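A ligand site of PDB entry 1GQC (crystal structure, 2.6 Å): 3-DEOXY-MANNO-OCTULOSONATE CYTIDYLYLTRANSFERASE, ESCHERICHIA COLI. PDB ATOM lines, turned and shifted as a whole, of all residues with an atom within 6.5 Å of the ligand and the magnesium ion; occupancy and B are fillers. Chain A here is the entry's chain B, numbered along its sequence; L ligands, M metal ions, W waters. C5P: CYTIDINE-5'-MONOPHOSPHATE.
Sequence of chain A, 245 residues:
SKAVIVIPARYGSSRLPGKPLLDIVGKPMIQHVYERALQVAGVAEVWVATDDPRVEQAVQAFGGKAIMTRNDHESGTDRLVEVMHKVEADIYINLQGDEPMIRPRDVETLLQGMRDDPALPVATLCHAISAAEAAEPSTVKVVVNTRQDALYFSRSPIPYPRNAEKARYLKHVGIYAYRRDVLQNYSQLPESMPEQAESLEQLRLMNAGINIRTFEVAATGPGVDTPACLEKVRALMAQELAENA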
ATOM      1  N   ILE A   7      -9.709   1.377   0.215  1.00  0.00           N
ATOM      2  CA  ILE A   7     -11.130   1.698   0.155  1.00  0.00           C
ATOM      3  C   ILE A   7     -11.890   1.060   1.315  1.00  0.00           C
ATOM      4  O   ILE A   7     -12.168  -0.140   1.289  1.00  0.00           O
ATOM      5  CB  ILE A   7     -11.761   1.167  -1.181  1.00  0.00           C
ATOM      6  CG1 ILE A   7     -10.996   1.733  -2.379  1.00  0.00           C
ATOM      7  CG2 ILE A   7     -13.214   1.588  -1.295  1.00  0.00           C
ATOM      8  CD1 ILE A   7     -11.303   1.063  -3.678  1.00  0.00           C
ATOM      9  N   PRO A   8     -12.246   1.839   2.351  1.00  0.00           N
ATOM     10  CA  PRO A   8     -12.981   1.267   3.486  1.00  0.00           C
ATOM     11  C   PRO A   8     -14.377   0.827   2.990  1.00  0.00           C
ATOM     12  O   PRO A   8     -15.124   1.655   2.436  1.00  0.00           O
ATOM     13  CB  PRO A   8     -13.061   2.421   4.473  1.00  0.00           C
ATOM     14  CG  PRO A   8     -11.903   3.290   4.104  1.00  0.00           C
ATOM     15  CD  PRO A   8     -11.913   3.248   2.604  1.00  0.00           C
ATOM     16  N   ALA A   9     -14.720  -0.453   3.141  1.00  0.00           N
ATOM     17  CA  ALA A   9     -16.027  -0.949   2.689  1.00  0.00           C
ATOM     18  C   ALA A   9     -16.695  -1.962   3.632  1.00  0.00           C
ATOM     19  O   ALA A   9     -16.854  -3.141   3.277  1.00  0.00           O
ATOM     20  CB  ALA A   9     -15.901  -1.568   1.277  1.00  0.00           C
ATOM     21  N   ARG A  10     -17.112  -1.493   4.805  1.00  0.00           N
ATOM     22  CA  ARG A  10     -17.776  -2.331   5.801  1.00  0.00           C
ATOM     23  C   ARG A  10     -19.131  -2.786   5.237  1.00  0.00           C
ATOM     24  O   ARG A  10     -19.784  -2.028   4.525  1.00  0.00           O
ATOM     25  CB  ARG A  10     -18.047  -1.523   7.079  1.00  0.00           C
ATOM     26  CG  ARG A  10     -19.079  -0.438   6.814  1.00  0.00           C
ATOM     27  CD  ARG A  10     -19.308   0.523   7.958  1.00  0.00           C
ATOM     28  NE  ARG A  10     -20.385   0.104   8.840  1.00  0.00           N
ATOM     29  CZ  ARG A  10     -21.299   0.931   9.340  1.00  0.00           C
ATOM     30  NH1 ARG A  10     -21.259   2.235   9.032  1.00  0.00           N
ATOM     31  NH2 ARG A  10     -22.242   0.460  10.141  1.00  0.00           N
ATOM     32  N   TYR A  11     -19.550  -3.996   5.595  1.00  0.00           N
ATOM     33  CA  TYR A  11     -20.822  -4.522   5.108  1.00  0.00           C
ATOM     34  C   TYR A  11     -22.012  -3.770   5.684  1.00  0.00           C
ATOM     35  O   TYR A  11     -22.984  -3.479   4.971  1.00  0.00           O
ATOM     36  CB  TYR A  11     -20.968  -5.988   5.475  1.00  0.00           C
ATOM     37  CG  TYR A  11     -22.269  -6.602   5.005  1.00  0.00           C
ATOM     38  CD1 TYR A  11     -22.423  -7.049   3.685  1.00  0.00           C
ATOM     39  CD2 TYR A  11     -23.361  -6.743   5.870  1.00  0.00           C
ATOM     40  CE1 TYR A  11     -23.615  -7.623   3.247  1.00  0.00           C
ATOM     41  CE2 TYR A  11     -24.559  -7.310   5.428  1.00  0.00           C
ATOM     42  CZ  TYR A  11     -24.680  -7.750   4.119  1.00  0.00           C
ATOM     43  OH  TYR A  11     -25.848  -8.319   3.678  1.00  0.00           O
ATOM     44  N   GLY A  12     -21.942  -3.479   6.983  1.00  0.00           N
ATOM     45  CA  GLY A  12     -23.032  -2.804   7.655  1.00  0.00           C
ATOM     46  C   GLY A  12     -23.303  -1.369   7.272  1.00  0.00           C
ATOM     47  O   GLY A  12     -22.410  -0.608   6.926  1.00  0.00           O
ATOM     48  N   SER A  13     -24.582  -1.001   7.341  1.00  0.00           N
ATOM     49  CA  SER A  13     -25.029   0.355   7.050  1.00  0.00           C
ATOM     50  C   SER A  13     -26.380   0.534   7.703  1.00  0.00           C
ATOM     51  O   SER A  13     -27.211  -0.366   7.732  1.00  0.00           O
ATOM     52  CB  SER A  13     -25.164   0.601   5.546  1.00  0.00           C
ATOM     53  OG  SER A  13     -25.707   1.886   5.310  1.00  0.00           O
ATOM     54  N   SER A  14     -26.604   1.732   8.218  1.00  0.00           N
ATOM     55  CA  SER A  14     -27.839   2.047   8.908  1.00  0.00           C
ATOM     56  C   SER A  14     -28.989   2.166   7.915  1.00  0.00           C
ATOM     57  O   SER A  14     -30.093   1.658   8.145  1.00  0.00           O
ATOM     58  CB  SER A  14     -27.633   3.369   9.652  1.00  0.00           C
ATOM     59  OG  SER A  14     -28.527   3.491  10.742  1.00  0.00           O
ATOM     60  N   LYS A  19     -24.416  -2.262   1.720  1.00  0.00           N
ATOM     61  CA  LYS A  19     -24.201  -1.205   0.723  1.00  0.00           C
ATOM     62  C   LYS A  19     -23.179  -1.492  -0.353  1.00  0.00           C
ATOM     63  O   LYS A  19     -23.443  -1.258  -1.524  1.00  0.00           O
ATOM     64  CB  LYS A  19     -23.831   0.117   1.407  1.00  0.00           C
ATOM     65  CG  LYS A  19     -24.425   1.347   0.709  1.00  0.00           C
ATOM     66  CD  LYS A  19     -23.747   2.652   1.087  1.00  0.00           C
ATOM     67  CE  LYS A  19     -23.719   2.894   2.585  1.00  0.00           C
ATOM     68  NZ  LYS A  19     -23.125   4.224   2.905  1.00  0.00           N
ATOM     69  N   PRO A  20     -21.993  -2.001   0.016  1.00  0.00           N
ATOM     70  CA  PRO A  20     -20.927  -2.309  -0.953  1.00  0.00           C
ATOM     71  C   PRO A  20     -21.357  -3.182  -2.105  1.00  0.00           C
ATOM     72  O   PRO A  20     -20.866  -3.042  -3.221  1.00  0.00           O
ATOM     73  CB  PRO A  20     -19.877  -2.993  -0.112  1.00  0.00           C
ATOM     74  CG  PRO A  20     -20.080  -2.386   1.242  1.00  0.00           C
ATOM     75  CD  PRO A  20     -21.570  -2.349   1.386  1.00  0.00           C
ATOM     76  N   ALA A  49     -10.682  -2.625   2.051  1.00  0.00           N
ATOM     77  CA  ALA A  49     -10.585  -3.056   3.427  1.00  0.00           C
ATOM     78  C   ALA A  49     -12.008  -3.335   3.896  1.00  0.00           C
ATOM     79  O   ALA A  49     -12.793  -2.408   4.066  1.00  0.00           O
ATOM     80  CB  ALA A  49      -9.948  -1.954   4.284  1.00  0.00           C
ATOM     81  N   ASP A  72     -15.075  -4.094  14.372  1.00  0.00           N
ATOM     82  CA  ASP A  72     -15.539  -3.173  15.395  1.00  0.00           C
ATOM     83  C   ASP A  72     -14.864  -1.815  15.328  1.00  0.00           C
ATOM     84  O   ASP A  72     -14.752  -1.124  16.336  1.00  0.00           O
ATOM     85  CB  ASP A  72     -15.335  -3.790  16.782  1.00  0.00           C
ATOM     86  CG  ASP A  72     -13.890  -3.875  17.172  1.00  0.00           C
ATOM     87  OD1 ASP A  72     -13.592  -4.525  18.199  1.00  0.00           O
ATOM     88  OD2 ASP A  72     -13.034  -3.301  16.471  1.00  0.00           O
ATOM     89  N   HIS A  73     -14.387  -1.448  14.151  1.00  0.00           N
ATOM     90  CA  HIS A  73     -13.767  -0.143  13.966  1.00  0.00           C
ATOM     91  C   HIS A  73     -14.893   0.879  13.961  1.00  0.00           C
ATOM     92  O   HIS A  73     -15.998   0.596  13.496  1.00  0.00           O
ATOM     93  CB  HIS A  73     -13.048  -0.085  12.636  1.00  0.00           C
ATOM     94  CG  HIS A  73     -11.672  -0.673  12.668  1.00  0.00           C
ATOM     95  ND1 HIS A  73     -10.648  -0.105  13.382  1.00  0.00           N
ATOM     96  CD2 HIS A  73     -11.169  -1.768  12.072  1.00  0.00           C
ATOM     97  CE1 HIS A  73      -9.551  -0.817  13.207  1.00  0.00           C
ATOM     98  NE2 HIS A  73      -9.835  -1.832  12.417  1.00  0.00           N
ATOM     99  N   GLU A  74     -14.606   2.070  14.478  1.00  0.00           N
ATOM    100  CA  GLU A  74     -15.611   3.125  14.554  1.00  0.00           C
ATOM    101  C   GLU A  74     -15.706   3.999  13.285  1.00  0.00           C
ATOM    102  O   GLU A  74     -16.646   4.770  13.116  1.00  0.00           O
ATOM    103  CB  GLU A  74     -15.322   4.003  15.761  1.00  0.00           C
ATOM    104  CG  GLU A  74     -15.090   3.231  17.049  1.00  0.00           C
ATOM    105  CD  GLU A  74     -16.352   2.520  17.543  1.00  0.00           C
ATOM    106  OE1 GLU A  74     -16.927   1.712  16.790  1.00  0.00           O
ATOM    107  OE2 GLU A  74     -16.753   2.775  18.688  1.00  0.00           O
ATOM    108  N   SER A  75     -14.738   3.883  12.383  1.00  0.00           N
ATOM    109  CA  SER A  75     -14.781   4.692  11.179  1.00  0.00           C
ATOM    110  C   SER A  75     -13.783   4.206  10.144  1.00  0.00           C
ATOM    111  O   SER A  75     -12.827   3.505  10.479  1.00  0.00           O
ATOM    112  CB  SER A  75     -14.506   6.161  11.507  1.00  0.00           C
ATOM    113  OG  SER A  75     -13.125   6.378  11.792  1.00  0.00           O
ATOM    114  N   GLY A  76     -14.017   4.568   8.894  1.00  0.00           N
ATOM    115  CA  GLY A  76     -13.110   4.164   7.843  1.00  0.00           C
ATOM    116  C   GLY A  76     -11.662   4.532   8.112  1.00  0.00           C
ATOM    117  O   GLY A  76     -10.759   3.815   7.705  1.00  0.00           O
ATOM    118  N   THR A  77     -11.428   5.651   8.776  1.00  0.00           N
ATOM    119  CA  THR A  77     -10.054   6.075   9.083  1.00  0.00           C
ATOM    120  C   THR A  77      -9.358   5.083  10.041  1.00  0.00           C
ATOM    121  O   THR A  77      -8.169   4.793   9.892  1.00  0.00           O
ATOM    122  CB  THR A  77     -10.031   7.487   9.731  1.00  0.00           C
ATOM    123  OG1 THR A  77     -10.482   8.455   8.780  1.00  0.00           O
ATOM    124  CG2 THR A  77      -8.637   7.834  10.190  1.00  0.00           C
ATOM    125  N   ARG A  79      -9.962   1.967  10.287  1.00  0.00           N
ATOM    126  CA  ARG A  79      -9.737   0.737   9.542  1.00  0.00           C
ATOM    127  C   ARG A  79      -8.502   0.964   8.657  1.00  0.00           C
ATOM    128  O   ARG A  79      -7.692   0.049   8.440  1.00  0.00           O
ATOM    129  CB  ARG A  79     -10.956   0.446   8.648  1.00  0.00           C
ATOM    130  CG  ARG A  79     -11.023  -0.960   8.058  1.00  0.00           C
ATOM    131  CD  ARG A  79     -12.283  -1.146   7.215  1.00  0.00           C
ATOM    132  NE  ARG A  79     -13.530  -0.854   7.938  1.00  0.00           N
ATOM    133  CZ  ARG A  79     -14.046  -1.633   8.879  1.00  0.00           C
ATOM    134  NH1 ARG A  79     -13.422  -2.757   9.209  1.00  0.00           N
ATOM    135  NH2 ARG A  79     -15.176  -1.311   9.487  1.00  0.00           N
ATOM    136  N   LEU A  95     -10.129   6.303  -0.178  1.00  0.00           N
ATOM    137  CA  LEU A  95     -11.238   6.543  -1.115  1.00  0.00           C
ATOM    138  C   LEU A  95     -12.523   6.001  -0.533  1.00  0.00           C
ATOM    139  O   LEU A  95     -12.585   4.839  -0.163  1.00  0.00           O
ATOM    140  CB  LEU A  95     -10.993   5.829  -2.443  1.00  0.00           C
ATOM    141  CG  LEU A  95     -10.096   6.439  -3.504  1.00  0.00           C
ATOM    142  CD1 LEU A  95      -9.909   5.453  -4.680  1.00  0.00           C
ATOM    143  CD2 LEU A  95     -10.743   7.716  -3.993  1.00  0.00           C
ATOM    144  N   GLN A  96     -13.574   6.818  -0.482  1.00  0.00           N
ATOM    145  CA  GLN A  96     -14.847   6.356   0.068  1.00  0.00           C
ATOM    146  C   GLN A  96     -15.426   5.221  -0.784  1.00  0.00           C
ATOM    147  O   GLN A  96     -15.425   5.266  -2.026  1.00  0.00           O
ATOM    148  CB  GLN A  96     -15.832   7.511   0.109  1.00  0.00           C
ATOM    149  CG  GLN A  96     -15.295   8.727   0.831  1.00  0.00           C
ATOM    150  CD  GLN A  96     -15.084   8.478   2.310  1.00  0.00           C
ATOM    151  OE1 GLN A  96     -16.043   8.294   3.058  1.00  0.00           O
ATOM    152  NE2 GLN A  96     -13.822   8.461   2.728  1.00  0.00           N
ATOM    153  N   GLY A  97     -15.948   4.193  -0.120  1.00  0.00           N
ATOM    154  CA  GLY A  97     -16.525   3.075  -0.833  1.00  0.00           C
ATOM    155  C   GLY A  97     -17.951   3.316  -1.312  1.00  0.00           C
ATOM    156  O   GLY A  97     -18.503   2.510  -2.045  1.00  0.00           O
ATOM    157  N   ASP A  98     -18.568   4.403  -0.897  1.00  0.00           N
ATOM    158  CA  ASP A  98     -19.924   4.656  -1.364  1.00  0.00           C
ATOM    159  C   ASP A  98     -19.996   5.838  -2.295  1.00  0.00           C
ATOM    160  O   ASP A  98     -21.042   6.450  -2.428  1.00  0.00           O
ATOM    161  CB  ASP A  98     -20.894   4.856  -0.186  1.00  0.00           C
ATOM    162  CG  ASP A  98     -20.325   5.706   0.934  1.00  0.00           C
ATOM    163  OD1 ASP A  98     -19.290   6.382   0.732  1.00  0.00           O
ATOM    164  OD2 ASP A  98     -20.923   5.709   2.037  1.00  0.00           O
ATOM    165  N   GLU A  99     -18.871   6.166  -2.936  1.00  0.00           N
ATOM    166  CA  GLU A  99     -18.799   7.261  -3.896  1.00  0.00           C
ATOM    167  C   GLU A  99     -18.219   6.702  -5.187  1.00  0.00           C
ATOM    168  O   GLU A  99     -17.020   6.830  -5.458  1.00  0.00           O
ATOM    169  CB  GLU A  99     -17.934   8.401  -3.353  1.00  0.00           C
ATOM    170  CG  GLU A  99     -18.721   9.472  -2.596  1.00  0.00           C
ATOM    171  CD  GLU A  99     -17.841  10.329  -1.688  1.00  0.00           C
ATOM    172  OE1 GLU A  99     -16.718  10.679  -2.118  1.00  0.00           O
ATOM    173  OE2 GLU A  99     -18.280  10.655  -0.560  1.00  0.00           O
ATOM    174  N   VAL A 224     -23.685   7.584  -2.152  1.00  0.00           N
ATOM    175  CA  VAL A 224     -24.760   6.624  -1.908  1.00  0.00           C
ATOM    176  C   VAL A 224     -24.992   6.351  -0.413  1.00  0.00           C
ATOM    177  O   VAL A 224     -24.398   5.431   0.169  1.00  0.00           O
ATOM    178  CB  VAL A 224     -24.451   5.270  -2.621  1.00  0.00           C
ATOM    179  CG1 VAL A 224     -25.504   4.221  -2.254  1.00  0.00           C
ATOM    180  CG2 VAL A 224     -24.417   5.475  -4.132  1.00  0.00           C
ATOM    181  N   ASP A 225     -25.848   7.158   0.199  1.00  0.00           N
ATOM    182  CA  ASP A 225     -26.141   7.006   1.616  1.00  0.00           C
ATOM    183  C   ASP A 225     -27.609   6.637   1.794  1.00  0.00           C
ATOM    184  O   ASP A 225     -27.969   5.971   2.748  1.00  0.00           O
ATOM    185  CB  ASP A 225     -25.872   8.318   2.373  1.00  0.00           C
ATOM    186  CG  ASP A 225     -24.675   9.090   1.833  1.00  0.00           C
ATOM    187  OD1 ASP A 225     -24.757   9.596   0.685  1.00  0.00           O
ATOM    188  OD2 ASP A 225     -23.659   9.201   2.558  1.00  0.00           O
HETATM  189  O3P C5P L   1     -21.159   4.322   6.327  1.00  0.00           O
HETATM  190  P   C5P L   1     -20.706   5.839   6.007  1.00  0.00           P
HETATM  191  O1P C5P L   1     -21.151   6.724   7.121  1.00  0.00           O
HETATM  192  O2P C5P L   1     -21.386   6.284   4.763  1.00  0.00           O
HETATM  193  O5' C5P L   1     -19.089   5.985   5.808  1.00  0.00           O
HETATM  194  C5' C5P L   1     -18.282   6.243   4.632  1.00  0.00           C
HETATM  195  C4' C5P L   1     -17.228   5.106   4.234  1.00  0.00           C
HETATM  196  O4' C5P L   1     -16.444   4.702   5.378  1.00  0.00           O
HETATM  197  C3' C5P L   1     -17.849   3.807   3.660  1.00  0.00           C
HETATM  198  O3' C5P L   1     -17.029   3.340   2.579  1.00  0.00           O
HETATM  199  C2' C5P L   1     -17.796   2.834   4.835  1.00  0.00           C
HETATM  200  O2' C5P L   1     -17.746   1.438   4.481  1.00  0.00           O
HETATM  201  C1' C5P L   1     -16.539   3.266   5.607  1.00  0.00           C
HETATM  202  N1  C5P L   1     -16.676   2.895   7.027  1.00  0.00           N
HETATM  203  C2  C5P L   1     -16.017   1.798   7.570  1.00  0.00           C
HETATM  204  N3  C5P L   1     -16.206   1.495   8.990  1.00  0.00           N
HETATM  205  C4  C5P L   1     -16.958   2.208   9.766  1.00  0.00           C
HETATM  206  C5  C5P L   1     -17.644   3.374   9.156  1.00  0.00           C
HETATM  207  C6  C5P L   1     -17.488   3.662   7.846  1.00  0.00           C
HETATM  208  O2  C5P L   1     -15.276   1.056   6.947  1.00  0.00           O
HETATM  209  N4  C5P L   1     -17.125   1.940  11.024  1.00  0.00           N
HETATM  210 MG    MG M   1     -21.481   7.960   3.390  1.00  0.00          MG
HETATM  211  O   HOH W   1     -20.669   9.551   1.941  1.00  0.00           O
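The backbone NH of Ser 75 lies close to a nitrogen (N4) of the ligand. CA of Ala 9 touches O2' of the ligand (3.4 Å). Glu 74 touches the ligand. Gly 76 touches the ligand. OE1 of Gln 96 touches C5' of the ligand, 3.4 Å away. Hydrophobic or aromatic side chains that line the ligand: Pro 8. 12 residues have an atom within 4 Å of the ligand: Pro 8, Ala 9, Arg 10, Lys 19, His 73, Glu 74, Ser 75, Gly 76, Arg 79, Gln 96, Gly 97 and Asp 98. Along chain A the residues within 4 Å of the ligand span positions 8 to 98.
OD2 of Asp 98 lies within salt-bridge range of NZ of Lys 19. The backbone carbonyl oxygen of Asp 98 is in hydrogen-bond range of the backbone NH of Val 224 (2.9 Å). NE of Arg 10 is in hydrogen-bond range of O of Gly 12, 2.9 Å away. The backbone carbonyl oxygen of Val 224 sits close to the side-chain amino group of Lys 19, 3.3 Å away. The backbone carbonyl oxygen (O) of Ala 49 sits at hydrogen-bond distance from the backbone NH (N) of Ala 9.
An oxygen (O3') of the ligand lies within hydrogen-bond range of the backbone carbonyl oxygen (O) of Pro 8. NE of Arg 79 lies within hydrogen-bond range of O2 of the ligand (2.8 Å). The backbone NH (N) of Arg 10 is in hydrogen-bond range of an oxygen (O2') of the ligand, 3.0 Å away. The guanidinium group (NH1) of Arg 10 lies within salt-bridge range of an oxygen (O3P) of the ligand (3.4 Å). O3' of the ligand lies within hydrogen-bond range of N of Gly 97, at 3.0 Å. The backbone carbonyl oxygen (O) of His 73 is in hydrogen-bond range of a nitrogen (N4) of the ligand (3.0 Å). The side-chain amino group of Lys 19 lies within salt-bridge range of an oxygen (O3P) of the ligand.
Two residues have an atom within 4 Å of the magnesium ion: Asp 98 and Asp 225. The nearest printed residue that does not touch the magnesium ion is Lys 19 (4.1 Å).
The magnesium ion is bound by an oxygen (O2P) of the ligand (2.2 Å) and water W1 (2.3 Å). Slightly farther from the magnesium ion lies the side-chain carboxylate (OD2) of Asp 225 (2.6 Å). Slightly farther from the magnesium ion lies OD2 of Asp 98 (2.7 Å).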
